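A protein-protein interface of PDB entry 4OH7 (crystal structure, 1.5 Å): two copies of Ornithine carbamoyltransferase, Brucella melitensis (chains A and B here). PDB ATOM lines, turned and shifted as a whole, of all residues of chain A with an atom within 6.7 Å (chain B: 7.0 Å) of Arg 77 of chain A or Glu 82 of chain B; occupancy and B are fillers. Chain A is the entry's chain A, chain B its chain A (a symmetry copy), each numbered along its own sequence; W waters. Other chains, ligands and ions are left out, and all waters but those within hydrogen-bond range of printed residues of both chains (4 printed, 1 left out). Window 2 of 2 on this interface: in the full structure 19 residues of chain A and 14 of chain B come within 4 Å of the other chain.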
ATOM      1  N   GLU A  49     -17.292  14.333   3.914  1.00  0.00           N
ATOM      2  CA  GLU A  49     -17.895  13.466   2.898  1.00  0.00           C
ATOM      3  C   GLU A  49     -19.338  13.225   3.261  1.00  0.00           C
ATOM      4  O   GLU A  49     -19.745  13.503   4.399  1.00  0.00           O
ATOM      5  CB  GLU A  49     -17.173  12.125   2.831  1.00  0.00           C
ATOM      6  CG  GLU A  49     -17.136  11.393   4.163  1.00  0.00           C
ATOM      7  CD  GLU A  49     -16.270  10.157   4.138  1.00  0.00           C
ATOM      8  OE1 GLU A  49     -15.013  10.295   4.007  1.00  0.00           O
ATOM      9  OE2 GLU A  49     -16.858   9.060   4.283  1.00  0.00           O
ATOM     10  N   ARG A  50     -20.116  12.718   2.302  1.00  0.00           N
ATOM     11  CA  ARG A  50     -21.553  12.575   2.505  1.00  0.00           C
ATOM     12  C   ARG A  50     -22.125  11.283   1.910  1.00  0.00           C
ATOM     13  O   ARG A  50     -23.082  11.329   1.142  1.00  0.00           O
ATOM     14  CB  ARG A  50     -22.289  13.814   1.963  1.00  0.00           C
ATOM     15  CG  ARG A  50     -21.794  15.152   2.510  1.00  0.00           C
ATOM     16  CD  ARG A  50     -22.539  16.344   1.896  1.00  0.00           C
ATOM     17  NE  ARG A  50     -23.990  16.167   1.986  1.00  0.00           N
ATOM     18  CZ  ARG A  50     -24.740  16.403   3.071  1.00  0.00           C
ATOM     19  NH1 ARG A  50     -24.213  16.869   4.204  1.00  0.00           N
ATOM     20  NH2 ARG A  50     -26.046  16.176   3.014  1.00  0.00           N
ATOM     21  N   MET A  59     -34.154  10.068  16.519  1.00  0.00           N
ATOM     22  CA  MET A  59     -33.532   9.787  17.811  1.00  0.00           C
ATOM     23  C   MET A  59     -34.583   9.914  18.889  1.00  0.00           C
ATOM     24  O   MET A  59     -35.008  11.011  19.176  1.00  0.00           O
ATOM     25  CB  MET A  59     -32.353  10.748  18.106  1.00  0.00           C
ATOM     26  CG  MET A  59     -31.307  10.800  16.995  1.00  0.00           C
ATOM     27  SD  MET A  59     -29.898  11.852  17.441  1.00  0.00           S
ATOM     28  CE  MET A  59     -30.721  13.429  17.748  1.00  0.00           C
ATOM     29  N   ARG A  69     -27.061  11.823  22.763  1.00  0.00           N
ATOM     30  CA  ARG A  69     -27.653  12.663  21.725  1.00  0.00           C
ATOM     31  C   ARG A  69     -26.574  13.343  20.908  1.00  0.00           C
ATOM     32  O   ARG A  69     -26.610  13.270  19.673  1.00  0.00           O
ATOM     33  CB  ARG A  69     -28.564  13.718  22.324  1.00  0.00           C
ATOM     34  CG  ARG A  69     -29.240  14.609  21.295  1.00  0.00           C
ATOM     35  CD  ARG A  69     -29.948  15.777  21.927  1.00  0.00           C
ATOM     36  NE  ARG A  69     -30.245  16.790  20.912  1.00  0.00           N
ATOM     37  CZ  ARG A  69     -30.681  18.000  21.179  1.00  0.00           C
ATOM     38  NH1 ARG A  69     -30.929  18.398  22.428  1.00  0.00           N
ATOM     39  NH2 ARG A  69     -30.909  18.815  20.168  1.00  0.00           N
ATOM     40  N   PHE A  72     -24.355  10.846  18.733  1.00  0.00           N
ATOM     41  CA  PHE A  72     -25.072  10.317  17.561  1.00  0.00           C
ATOM     42  C   PHE A  72     -25.368  11.417  16.541  1.00  0.00           C
ATOM     43  O   PHE A  72     -25.284  11.178  15.334  1.00  0.00           O
ATOM     44  CB  PHE A  72     -26.414   9.655  17.955  1.00  0.00           C
ATOM     45  CG  PHE A  72     -26.338   8.173  18.157  1.00  0.00           C
ATOM     46  CD1 PHE A  72     -26.304   7.328  17.067  1.00  0.00           C
ATOM     47  CD2 PHE A  72     -26.268   7.620  19.423  1.00  0.00           C
ATOM     48  CE1 PHE A  72     -26.225   5.960  17.218  1.00  0.00           C
ATOM     49  CE2 PHE A  72     -26.196   6.258  19.590  1.00  0.00           C
ATOM     50  CZ  PHE A  72     -26.161   5.433  18.485  1.00  0.00           C
ATOM     51  N   ASP A  73     -25.750  12.619  16.979  1.00  0.00           N
ATOM     52  CA  ASP A  73     -26.154  13.688  16.077  1.00  0.00           C
ATOM     53  C   ASP A  73     -24.973  14.100  15.201  1.00  0.00           C
ATOM     54  O   ASP A  73     -25.063  14.136  13.973  1.00  0.00           O
ATOM     55  CB  ASP A  73     -26.650  14.858  16.920  1.00  0.00           C
ATOM     56  CG  ASP A  73     -27.427  15.857  16.151  1.00  0.00           C
ATOM     57  OD1 ASP A  73     -27.679  15.641  14.967  1.00  0.00           O
ATOM     58  OD2 ASP A  73     -27.819  16.894  16.751  1.00  0.00           O
ATOM     59  N   VAL A  74     -23.850  14.356  15.847  1.00  0.00           N
ATOM     60  CA  VAL A  74     -22.680  14.775  15.094  1.00  0.00           C
ATOM     61  C   VAL A  74     -22.254  13.664  14.147  1.00  0.00           C
ATOM     62  O   VAL A  74     -21.864  13.937  13.015  1.00  0.00           O
ATOM     63  CB  VAL A  74     -21.509  15.183  16.035  1.00  0.00           C
ATOM     64  CG1 VAL A  74     -20.238  15.420  15.213  1.00  0.00           C
ATOM     65  CG2 VAL A  74     -21.876  16.417  16.859  1.00  0.00           C
ATOM     66  N   GLY A  75     -22.247  12.426  14.619  1.00  0.00           N
ATOM     67  CA  GLY A  75     -21.855  11.285  13.789  1.00  0.00           C
ATOM     68  C   GLY A  75     -22.693  11.130  12.539  1.00  0.00           C
ATOM     69  O   GLY A  75     -22.176  11.012  11.430  1.00  0.00           O
ATOM     70  N   MET A  76     -24.007  11.209  12.697  1.00  0.00           N
ATOM     71  CA  MET A  76     -24.900  11.113  11.535  1.00  0.00           C
ATOM     72  C   MET A  76     -24.661  12.250  10.549  1.00  0.00           C
ATOM     73  O   MET A  76     -24.593  12.033   9.328  1.00  0.00           O
ATOM     74  CB  MET A  76     -26.367  11.096  11.989  1.00  0.00           C
ATOM     75  CG  MET A  76     -27.360  10.888  10.861  1.00  0.00           C
ATOM     76  SD  MET A  76     -27.191   9.248  10.091  1.00  0.00           S
ATOM     77  CE  MET A  76     -28.632   9.294   8.995  1.00  0.00           C
ATOM     78  N   ARG A  77     -24.432  13.452  11.060  1.00  0.00           N
ATOM     79  CA  ARG A  77     -24.197  14.581  10.186  1.00  0.00           C
ATOM     80  C   ARG A  77     -22.897  14.444   9.417  1.00  0.00           C
ATOM     81  O   ARG A  77     -22.831  14.812   8.241  1.00  0.00           O
ATOM     82  CB  ARG A  77     -24.265  15.864  10.958  1.00  0.00           C
ATOM     83  CG  ARG A  77     -25.649  16.073  11.532  1.00  0.00           C
ATOM     84  CD  ARG A  77     -25.719  17.448  12.096  1.00  0.00           C
ATOM     85  NE  ARG A  77     -26.733  17.560  13.142  1.00  0.00           N
ATOM     86  CZ  ARG A  77     -27.420  18.665  13.398  1.00  0.00           C
ATOM     87  NH1 ARG A  77     -27.243  19.765  12.674  1.00  0.00           N
ATOM     88  NH2 ARG A  77     -28.311  18.651  14.395  1.00  0.00           N
ATOM     89  N   GLN A  78     -21.881  13.897  10.079  1.00  0.00           N
ATOM     90  CA  GLN A  78     -20.596  13.650   9.398  1.00  0.00           C
ATOM     91  C   GLN A  78     -20.710  12.584   8.318  1.00  0.00           C
ATOM     92  O   GLN A  78     -19.900  12.552   7.397  1.00  0.00           O
ATOM     93  CB  GLN A  78     -19.523  13.275  10.424  1.00  0.00           C
ATOM     94  CG  GLN A  78     -19.080  14.455  11.274  1.00  0.00           C
ATOM     95  CD  GLN A  78     -18.023  14.112  12.275  1.00  0.00           C
ATOM     96  OE1 GLN A  78     -17.694  12.936  12.482  1.00  0.00           O
ATOM     97  NE2 GLN A  78     -17.504  15.120  12.943  1.00  0.00           N
ATOM     98  N   LEU A  79     -21.699  11.700   8.406  1.00  0.00           N
ATOM     99  CA  LEU A  79     -21.988  10.774   7.313  1.00  0.00           C
ATOM    100  C   LEU A  79     -22.783  11.420   6.165  1.00  0.00           C
ATOM    101  O   LEU A  79     -23.060  10.758   5.163  1.00  0.00           O
ATOM    102  CB  LEU A  79     -22.785   9.584   7.832  1.00  0.00           C
ATOM    103  CG  LEU A  79     -22.041   8.662   8.787  1.00  0.00           C
ATOM    104  CD1 LEU A  79     -23.016   7.616   9.322  1.00  0.00           C
ATOM    105  CD2 LEU A  79     -20.865   8.021   8.042  1.00  0.00           C
ATOM    106  N   GLY A  80     -23.186  12.670   6.370  1.00  0.00           N
ATOM    107  CA  GLY A  80     -24.012  13.428   5.442  1.00  0.00           C
ATOM    108  C   GLY A  80     -25.495  13.305   5.682  1.00  0.00           C
ATOM    109  O   GLY A  80     -26.280  13.841   4.903  1.00  0.00           O
ATOM    110  N   GLY A  81     -25.891  12.609   6.751  1.00  0.00           N
ATOM    111  CA  GLY A  81     -27.305  12.447   7.039  1.00  0.00           C
ATOM    112  C   GLY A  81     -27.894  13.533   7.920  1.00  0.00           C
ATOM    113  O   GLY A  81     -27.245  14.520   8.281  1.00  0.00           O
ATOM    114  N   GLU A  82     -29.160  13.313   8.241  1.00  0.00           N
ATOM    115  CA  GLU A  82     -30.008  14.212   8.984  1.00  0.00           C
ATOM    116  C   GLU A  82     -30.435  13.523  10.264  1.00  0.00           C
ATOM    117  O   GLU A  82     -30.561  12.314  10.290  1.00  0.00           O
ATOM    118  CB  GLU A  82     -31.320  14.442   8.217  1.00  0.00           C
ATOM    119  CG  GLU A  82     -31.221  14.773   6.733  1.00  0.00           C
ATOM    120  CD  GLU A  82     -30.623  16.139   6.469  1.00  0.00           C
ATOM    121  OE1 GLU A  82     -30.466  16.939   7.428  1.00  0.00           O
ATOM    122  OE2 GLU A  82     -30.264  16.403   5.293  1.00  0.00           O
ATOM    123  N   THR A  83     -30.715  14.300  11.298  1.00  0.00           N
ATOM    124  CA  THR A  83     -31.243  13.759  12.546  1.00  0.00           C
ATOM    125  C   THR A  83     -32.465  14.524  12.990  1.00  0.00           C
ATOM    126  O   THR A  83     -32.602  15.702  12.709  1.00  0.00           O
ATOM    127  CB  THR A  83     -30.207  13.849  13.680  1.00  0.00           C
ATOM    128  OG1 THR A  83     -29.988  15.233  13.976  1.00  0.00           O
ATOM    129  CG2 THR A  83     -28.892  13.238  13.238  1.00  0.00           C
ATOM    130  N   LEU A 309     -23.923   3.320  12.712  1.00  0.00           N
ATOM    131  CA  LEU A 309     -24.909   3.923  11.802  1.00  0.00           C
ATOM    132  C   LEU A 309     -24.652   3.489  10.357  1.00  0.00           C
ATOM    133  O   LEU A 309     -25.570   3.113   9.659  1.00  0.00           O
ATOM    134  CB  LEU A 309     -24.849   5.436  11.904  1.00  0.00           C
ATOM    135  CG  LEU A 309     -25.472   6.069  13.157  1.00  0.00           C
ATOM    136  CD1 LEU A 309     -25.016   7.510  13.287  1.00  0.00           C
ATOM    137  CD2 LEU A 309     -26.988   6.017  13.145  1.00  0.00           C
ATOM    138  N   ARG B  50     -20.559  27.520   1.713  1.00  0.00           N
ATOM    139  CA  ARG B  50     -20.375  26.621   2.846  1.00  0.00           C
ATOM    140  C   ARG B  50     -18.931  26.575   3.358  1.00  0.00           C
ATOM    141  O   ARG B  50     -18.354  25.497   3.480  1.00  0.00           O
ATOM    142  CB  ARG B  50     -20.887  25.213   2.491  1.00  0.00           C
ATOM    143  CG  ARG B  50     -22.327  25.157   1.980  1.00  0.00           C
ATOM    144  CD  ARG B  50     -22.758  23.735   1.604  1.00  0.00           C
ATOM    145  NE  ARG B  50     -22.476  22.790   2.686  1.00  0.00           N
ATOM    146  CZ  ARG B  50     -23.230  22.607   3.779  1.00  0.00           C
ATOM    147  NH1 ARG B  50     -24.368  23.275   3.970  1.00  0.00           N
ATOM    148  NH2 ARG B  50     -22.839  21.728   4.693  1.00  0.00           N
ATOM    149  N   TYR B  52     -17.730  26.802   6.336  1.00  0.00           N
ATOM    150  CA  TYR B  52     -17.583  26.038   7.555  1.00  0.00           C
ATOM    151  C   TYR B  52     -18.396  24.751   7.522  1.00  0.00           C
ATOM    152  O   TYR B  52     -18.830  24.254   8.553  1.00  0.00           O
ATOM    153  CB  TYR B  52     -17.896  26.921   8.778  1.00  0.00           C
ATOM    154  CG  TYR B  52     -16.861  28.011   8.900  1.00  0.00           C
ATOM    155  CD1 TYR B  52     -15.557  27.697   9.292  1.00  0.00           C
ATOM    156  CD2 TYR B  52     -17.152  29.306   8.532  1.00  0.00           C
ATOM    157  CE1 TYR B  52     -14.570  28.668   9.343  1.00  0.00           C
ATOM    158  CE2 TYR B  52     -16.181  30.297   8.580  1.00  0.00           C
ATOM    159  CZ  TYR B  52     -14.893  29.957   8.996  1.00  0.00           C
ATOM    160  OH  TYR B  52     -13.911  30.942   9.049  1.00  0.00           O
ATOM    161  N   ALA B  53     -18.522  24.154   6.334  1.00  0.00           N
ATOM    162  CA  ALA B  53     -19.044  22.782   6.219  1.00  0.00           C
ATOM    163  C   ALA B  53     -18.344  21.830   7.189  1.00  0.00           C
ATOM    164  O   ALA B  53     -17.128  21.891   7.341  1.00  0.00           O
ATOM    165  CB  ALA B  53     -18.892  22.287   4.767  1.00  0.00           C
ATOM    166  N   GLY B  54     -19.115  20.997   7.901  1.00  0.00           N
ATOM    167  CA  GLY B  54     -18.556  20.058   8.871  1.00  0.00           C
ATOM    168  C   GLY B  54     -18.256  20.619  10.257  1.00  0.00           C
ATOM    169  O   GLY B  54     -17.713  19.904  11.108  1.00  0.00           O
ATOM    170  N   LYS B  55     -18.502  21.911  10.458  1.00  0.00           N
ATOM    171  CA  LYS B  55     -18.340  22.514  11.776  1.00  0.00           C
ATOM    172  C   LYS B  55     -19.692  22.453  12.477  1.00  0.00           C
ATOM    173  O   LYS B  55     -20.739  22.619  11.840  1.00  0.00           O
ATOM    174  CB  LYS B  55     -17.857  23.964  11.696  1.00  0.00           C
ATOM    175  CG  LYS B  55     -16.504  24.154  11.005  1.00  0.00           C
ATOM    176  CD  LYS B  55     -15.332  23.642  11.832  1.00  0.00           C
ATOM    177  CE  LYS B  55     -14.019  23.775  11.033  1.00  0.00           C
ATOM    178  NZ  LYS B  55     -12.808  23.603  11.892  1.00  0.00           N
ATOM    179  N   VAL B  56     -19.651  22.198  13.779  1.00  0.00           N
ATOM    180  CA  VAL B  56     -20.834  22.117  14.632  1.00  0.00           C
ATOM    181  C   VAL B  56     -20.784  23.113  15.772  1.00  0.00           C
ATOM    182  O   VAL B  56     -19.793  23.236  16.498  1.00  0.00           O
ATOM    183  CB  VAL B  56     -21.067  20.692  15.190  1.00  0.00           C
ATOM    184  CG1 VAL B  56     -22.315  20.648  16.061  1.00  0.00           C
ATOM    185  CG2 VAL B  56     -21.165  19.671  14.080  1.00  0.00           C
ATOM    186  N   LEU B  57     -21.886  23.826  15.930  1.00  0.00           N
ATOM    187  CA  LEU B  57     -22.095  24.753  17.040  1.00  0.00           C
ATOM    188  C   LEU B  57     -23.075  24.142  18.048  1.00  0.00           C
ATOM    189  O   LEU B  57     -24.233  23.862  17.693  1.00  0.00           O
ATOM    190  CB  LEU B  57     -22.687  26.063  16.511  1.00  0.00           C
ATOM    191  CG  LEU B  57     -23.034  27.113  17.561  1.00  0.00           C
ATOM    192  CD1 LEU B  57     -21.800  27.751  18.182  1.00  0.00           C
ATOM    193  CD2 LEU B  57     -23.902  28.184  16.901  1.00  0.00           C
ATOM    194  N   ALA B  58     -22.611  23.892  19.271  1.00  0.00           N
ATOM    195  CA  ALA B  58     -23.520  23.582  20.367  1.00  0.00           C
ATOM    196  C   ALA B  58     -24.126  24.866  20.889  1.00  0.00           C
ATOM    197  O   ALA B  58     -23.418  25.870  21.072  1.00  0.00           O
ATOM    198  CB  ALA B  58     -22.793  22.842  21.483  1.00  0.00           C
ATOM    199  N   MET B  59     -25.440  24.872  21.088  1.00  0.00           N
ATOM    200  CA  MET B  59     -26.117  26.055  21.615  1.00  0.00           C
ATOM    201  C   MET B  59     -26.740  25.701  22.945  1.00  0.00           C
ATOM    202  O   MET B  59     -27.704  24.968  22.970  1.00  0.00           O
ATOM    203  CB  MET B  59     -27.202  26.580  20.644  1.00  0.00           C
ATOM    204  CG  MET B  59     -26.695  26.828  19.225  1.00  0.00           C
ATOM    205  SD  MET B  59     -27.978  27.544  18.163  1.00  0.00           S
ATOM    206  CE  MET B  59     -29.268  26.288  18.272  1.00  0.00           C
ATOM    207  N   ASP B  73     -28.856  30.021  14.831  1.00  0.00           N
ATOM    208  CA  ASP B  73     -29.059  28.782  14.095  1.00  0.00           C
ATOM    209  C   ASP B  73     -28.994  29.055  12.594  1.00  0.00           C
ATOM    210  O   ASP B  73     -28.242  28.417  11.855  1.00  0.00           O
ATOM    211  CB  ASP B  73     -30.416  28.212  14.493  1.00  0.00           C
ATOM    212  CG  ASP B  73     -30.596  26.792  14.115  1.00  0.00           C
ATOM    213  OD1 ASP B  73     -29.657  26.178  13.611  1.00  0.00           O
ATOM    214  OD2 ASP B  73     -31.714  26.254  14.343  1.00  0.00           O
ATOM    215  N   MET B  76     -25.342  30.084  11.512  1.00  0.00           N
ATOM    216  CA  MET B  76     -24.420  28.947  11.396  1.00  0.00           C
ATOM    217  C   MET B  76     -24.712  28.112  10.156  1.00  0.00           C
ATOM    218  O   MET B  76     -23.793  27.719   9.419  1.00  0.00           O
ATOM    219  CB  MET B  76     -24.486  28.075  12.659  1.00  0.00           C
ATOM    220  CG  MET B  76     -23.484  26.936  12.677  1.00  0.00           C
ATOM    221  SD  MET B  76     -21.765  27.533  12.727  1.00  0.00           S
ATOM    222  CE  MET B  76     -20.917  25.950  12.958  1.00  0.00           C
ATOM    223  N   ARG B  77     -25.987  27.911   9.853  1.00  0.00           N
ATOM    224  CA  ARG B  77     -26.343  27.128   8.690  1.00  0.00           C
ATOM    225  C   ARG B  77     -25.938  27.811   7.398  1.00  0.00           C
ATOM    226  O   ARG B  77     -25.497  27.145   6.457  1.00  0.00           O
ATOM    227  CB  ARG B  77     -27.801  26.784   8.716  1.00  0.00           C
ATOM    228  CG  ARG B  77     -28.128  25.915   9.909  1.00  0.00           C
ATOM    229  CD  ARG B  77     -29.529  25.431   9.768  1.00  0.00           C
ATOM    230  NE  ARG B  77     -30.126  25.097  11.058  1.00  0.00           N
ATOM    231  CZ  ARG B  77     -31.040  24.153  11.233  1.00  0.00           C
ATOM    232  NH1 ARG B  77     -31.459  23.407  10.216  1.00  0.00           N
ATOM    233  NH2 ARG B  77     -31.527  23.950  12.462  1.00  0.00           N
ATOM    234  N   LEU B  79     -23.364  29.611   7.058  1.00  0.00           N
ATOM    235  CA  LEU B  79     -21.929  29.367   6.920  1.00  0.00           C
ATOM    236  C   LEU B  79     -21.600  27.938   6.453  1.00  0.00           C
ATOM    237  O   LEU B  79     -20.427  27.612   6.260  1.00  0.00           O
ATOM    238  CB  LEU B  79     -21.227  29.606   8.250  1.00  0.00           C
ATOM    239  CG  LEU B  79     -21.217  31.048   8.738  1.00  0.00           C
ATOM    240  CD1 LEU B  79     -20.611  31.089  10.138  1.00  0.00           C
ATOM    241  CD2 LEU B  79     -20.423  31.900   7.744  1.00  0.00           C
ATOM    242  N   GLY B  80     -22.633  27.108   6.350  1.00  0.00           N
ATOM    243  CA  GLY B  80     -22.522  25.701   5.999  1.00  0.00           C
ATOM    244  C   GLY B  80     -22.371  24.773   7.178  1.00  0.00           C
ATOM    245  O   GLY B  80     -22.189  23.574   6.984  1.00  0.00           O
ATOM    246  N   GLY B  81     -22.448  25.309   8.399  1.00  0.00           N
ATOM    247  CA  GLY B  81     -22.307  24.475   9.578  1.00  0.00           C
ATOM    248  C   GLY B  81     -23.609  23.894  10.096  1.00  0.00           C
ATOM    249  O   GLY B  81     -24.684  24.044   9.506  1.00  0.00           O
ATOM    250  N   GLU B  82     -23.465  23.213  11.222  1.00  0.00           N
ATOM    251  CA  GLU B  82     -24.502  22.471  11.895  1.00  0.00           C
ATOM    252  C   GLU B  82     -24.712  23.076  13.268  1.00  0.00           C
ATOM    253  O   GLU B  82     -23.780  23.599  13.851  1.00  0.00           O
ATOM    254  CB  GLU B  82     -24.018  21.040  12.179  1.00  0.00           C
ATOM    255  CG  GLU B  82     -23.361  20.278  11.034  1.00  0.00           C
ATOM    256  CD  GLU B  82     -24.330  19.920   9.927  1.00  0.00           C
ATOM    257  OE1 GLU B  82     -25.564  20.068  10.117  1.00  0.00           O
ATOM    258  OE2 GLU B  82     -23.850  19.523   8.835  1.00  0.00           O
ATOM    259  N   THR B  83     -25.915  22.948  13.804  1.00  0.00           N
ATOM    260  CA  THR B  83     -26.204  23.390  15.163  1.00  0.00           C
ATOM    261  C   THR B  83     -26.900  22.305  15.946  1.00  0.00           C
ATOM    262  O   THR B  83     -27.612  21.488  15.387  1.00  0.00           O
ATOM    263  CB  THR B  83     -27.126  24.623  15.169  1.00  0.00           C
ATOM    264  OG1 THR B  83     -28.404  24.227  14.662  1.00  0.00           O
ATOM    265  CG2 THR B  83     -26.562  25.702  14.264  1.00  0.00           C
ATOM    266  N   ILE B  84     -26.696  22.331  17.259  1.00  0.00           N
ATOM    267  CA  ILE B  84     -27.374  21.423  18.180  1.00  0.00           C
ATOM    268  C   ILE B  84     -27.950  22.267  19.314  1.00  0.00           C
ATOM    269  O   ILE B  84     -27.221  22.931  20.038  1.00  0.00           O
ATOM    270  CB  ILE B  84     -26.420  20.342  18.740  1.00  0.00           C
ATOM    271  CG1 ILE B  84     -25.822  19.507  17.597  1.00  0.00           C
ATOM    272  CG2 ILE B  84     -27.155  19.429  19.722  1.00  0.00           C
ATOM    273  CD1 ILE B  84     -24.800  18.479  18.065  1.00  0.00           C
ATOM    274  N   MET B  85     -29.273  22.254  19.446  1.00  0.00           N
ATOM    275  CA  MET B  85     -29.988  23.016  20.481  1.00  0.00           C
ATOM    276  C   MET B  85     -30.086  22.226  21.777  1.00  0.00           C
ATOM    277  O   MET B  85     -30.661  21.125  21.775  1.00  0.00           O
ATOM    278  CB  MET B  85     -31.424  23.328  19.966  1.00  0.00           C
ATOM    279  CG  MET B  85     -32.366  23.989  20.931  1.00  0.00           C
ATOM    280  SD  MET B  85     -31.740  25.555  21.489  1.00  0.00           S
ATOM    281  CE  MET B  85     -32.897  25.880  22.813  1.00  0.00           C
HETATM  282  O   HOH W   1     -18.621  17.706  12.580  1.00  0.00           O
HETATM  283  O   HOH W   2     -30.764  20.579  17.480  1.00  0.00           O
HETATM  284  O   HOH W   3     -28.108  22.248  12.022  1.00  0.00           O
HETATM  285  O   HOH W   4     -28.526  18.326   9.473  1.00  0.00           O
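Printed residues of chain B within 4 Å of Arg 69 of chain A: Ile 84 (3.8 Å) and Met 85 (2.8 Å). Phe 72 of chain A touches none of the printed residues of chain B. Arg 77 of chain A touches just these residues of chain B: Glu 82 and Thr 83. Of chain A, only Arg 77 comes within 4 Å of Glu 82 of chain B. Of the printed residues of chain A, Ile 84 of chain B touches Arg 69 (3.8 Å), Asp 73 (3.4 Å) and Val 74 (3.8 Å). The nearest residue of chain B that does not touch Arg 77 of chain A is Ile 84 of chain B (4.1 Å). The nearest residue of chain A that does not touch Glu 82 of chain B is Arg 50 of chain A (5.3 Å).
Among the printed residues, merely in contact across the chains: Asp 73 of chain A with Ile 84 of chain B (3.4 Å), Val 74 of chain A with Ile 84 of chain B (3.8 Å) and Arg 69 of chain A with Ile 84 of chain B (3.8 Å).
Hydrophobic or aromatic side chains of chain A within 4 Å of the printed part of chain B: Val 74. Along chain A the printed residues that touch a printed residue of chain B span positions 69 to 77. Among the printed residues, 6 pairs touch across the chains. Among the printed residues, Asp or Glu carboxylates within 4 Å of a Lys or Arg side-chain nitrogen of the other chain: Arg 77 of chain A with Glu 82 of chain B.
Water W3 lies within hydrogen-bond range of the guanidinium group of Arg 77 of chain A (2.7 Å) and the backbone NH of Thr 83 of chain B (2.9 Å). Water W1 lies within hydrogen-bond range of O of Gly 54 of chain B and NE2 of Gln 78 of chain A. Water W2 bridges N of Met 85 of chain B (3.0 Å) and NH2 of Arg 69 of chain A (3.2 Å). Water W4 bridges OE1 of Glu 82 of chain A and OE1 of Glu 82 of chain B.
Arg 77 of chain A touches Glu 82 of chain B, but with the chains exchanged Glu 82 of chain A does not touch Arg 77 of chain B (7.1 Å). Arg 77 of chain A touches Thr 83 of chain B, but with the chains exchanged Thr 83 of chain A does not touch Arg 77 of chain B (8.2 Å). Of the 6 pairs that touch across the chains among the printed residues, none has its exchanged pair printed and touching as well.
The guanidinium group (NH2) of Arg 77 of chain A sits at hydrogen-bond distance from the backbone carbonyl oxygen (O) of Thr 83 of chain B. The guanidinium group (NH1) of Arg 77 of chain A lies within salt-bridge range of the side-chain carboxylate (OE1) of Glu 82 of chain B (3.1 Å). The backbone carbonyl oxygen (O) of Met 85 of chain B sits at hydrogen-bond distance from the guanidinium group (NH1) of Arg 69 of chain A, 2.8 Å away.
The guanidinium group of Arg 77 of chain A lies within salt-bridge range of the side-chain carboxylate of Asp 73 of chain A, 2.8 Å away. The backbone carbonyl oxygen (O) of Leu 57 of chain B is in hydrogen-bond range of the backbone NH (N) of Ile 84 of chain B, 2.9 Å away. N of Glu 82 of chain B sits at hydrogen-bond distance from O of Lys 55 of chain B, 2.9 Å away. O of Ile 84 of chain B lies within hydrogen-bond range of N of Met 59 of chain B, 2.8 Å away. O of Glu 82 of chain B is in hydrogen-bond range of N of Leu 57 of chain B, 2.8 Å away. The side-chain carboxylate of Asp 73 of chain A lies within hydrogen-bond range of the side-chain hydroxyl of Thr 83 of chain A (2.5 Å).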
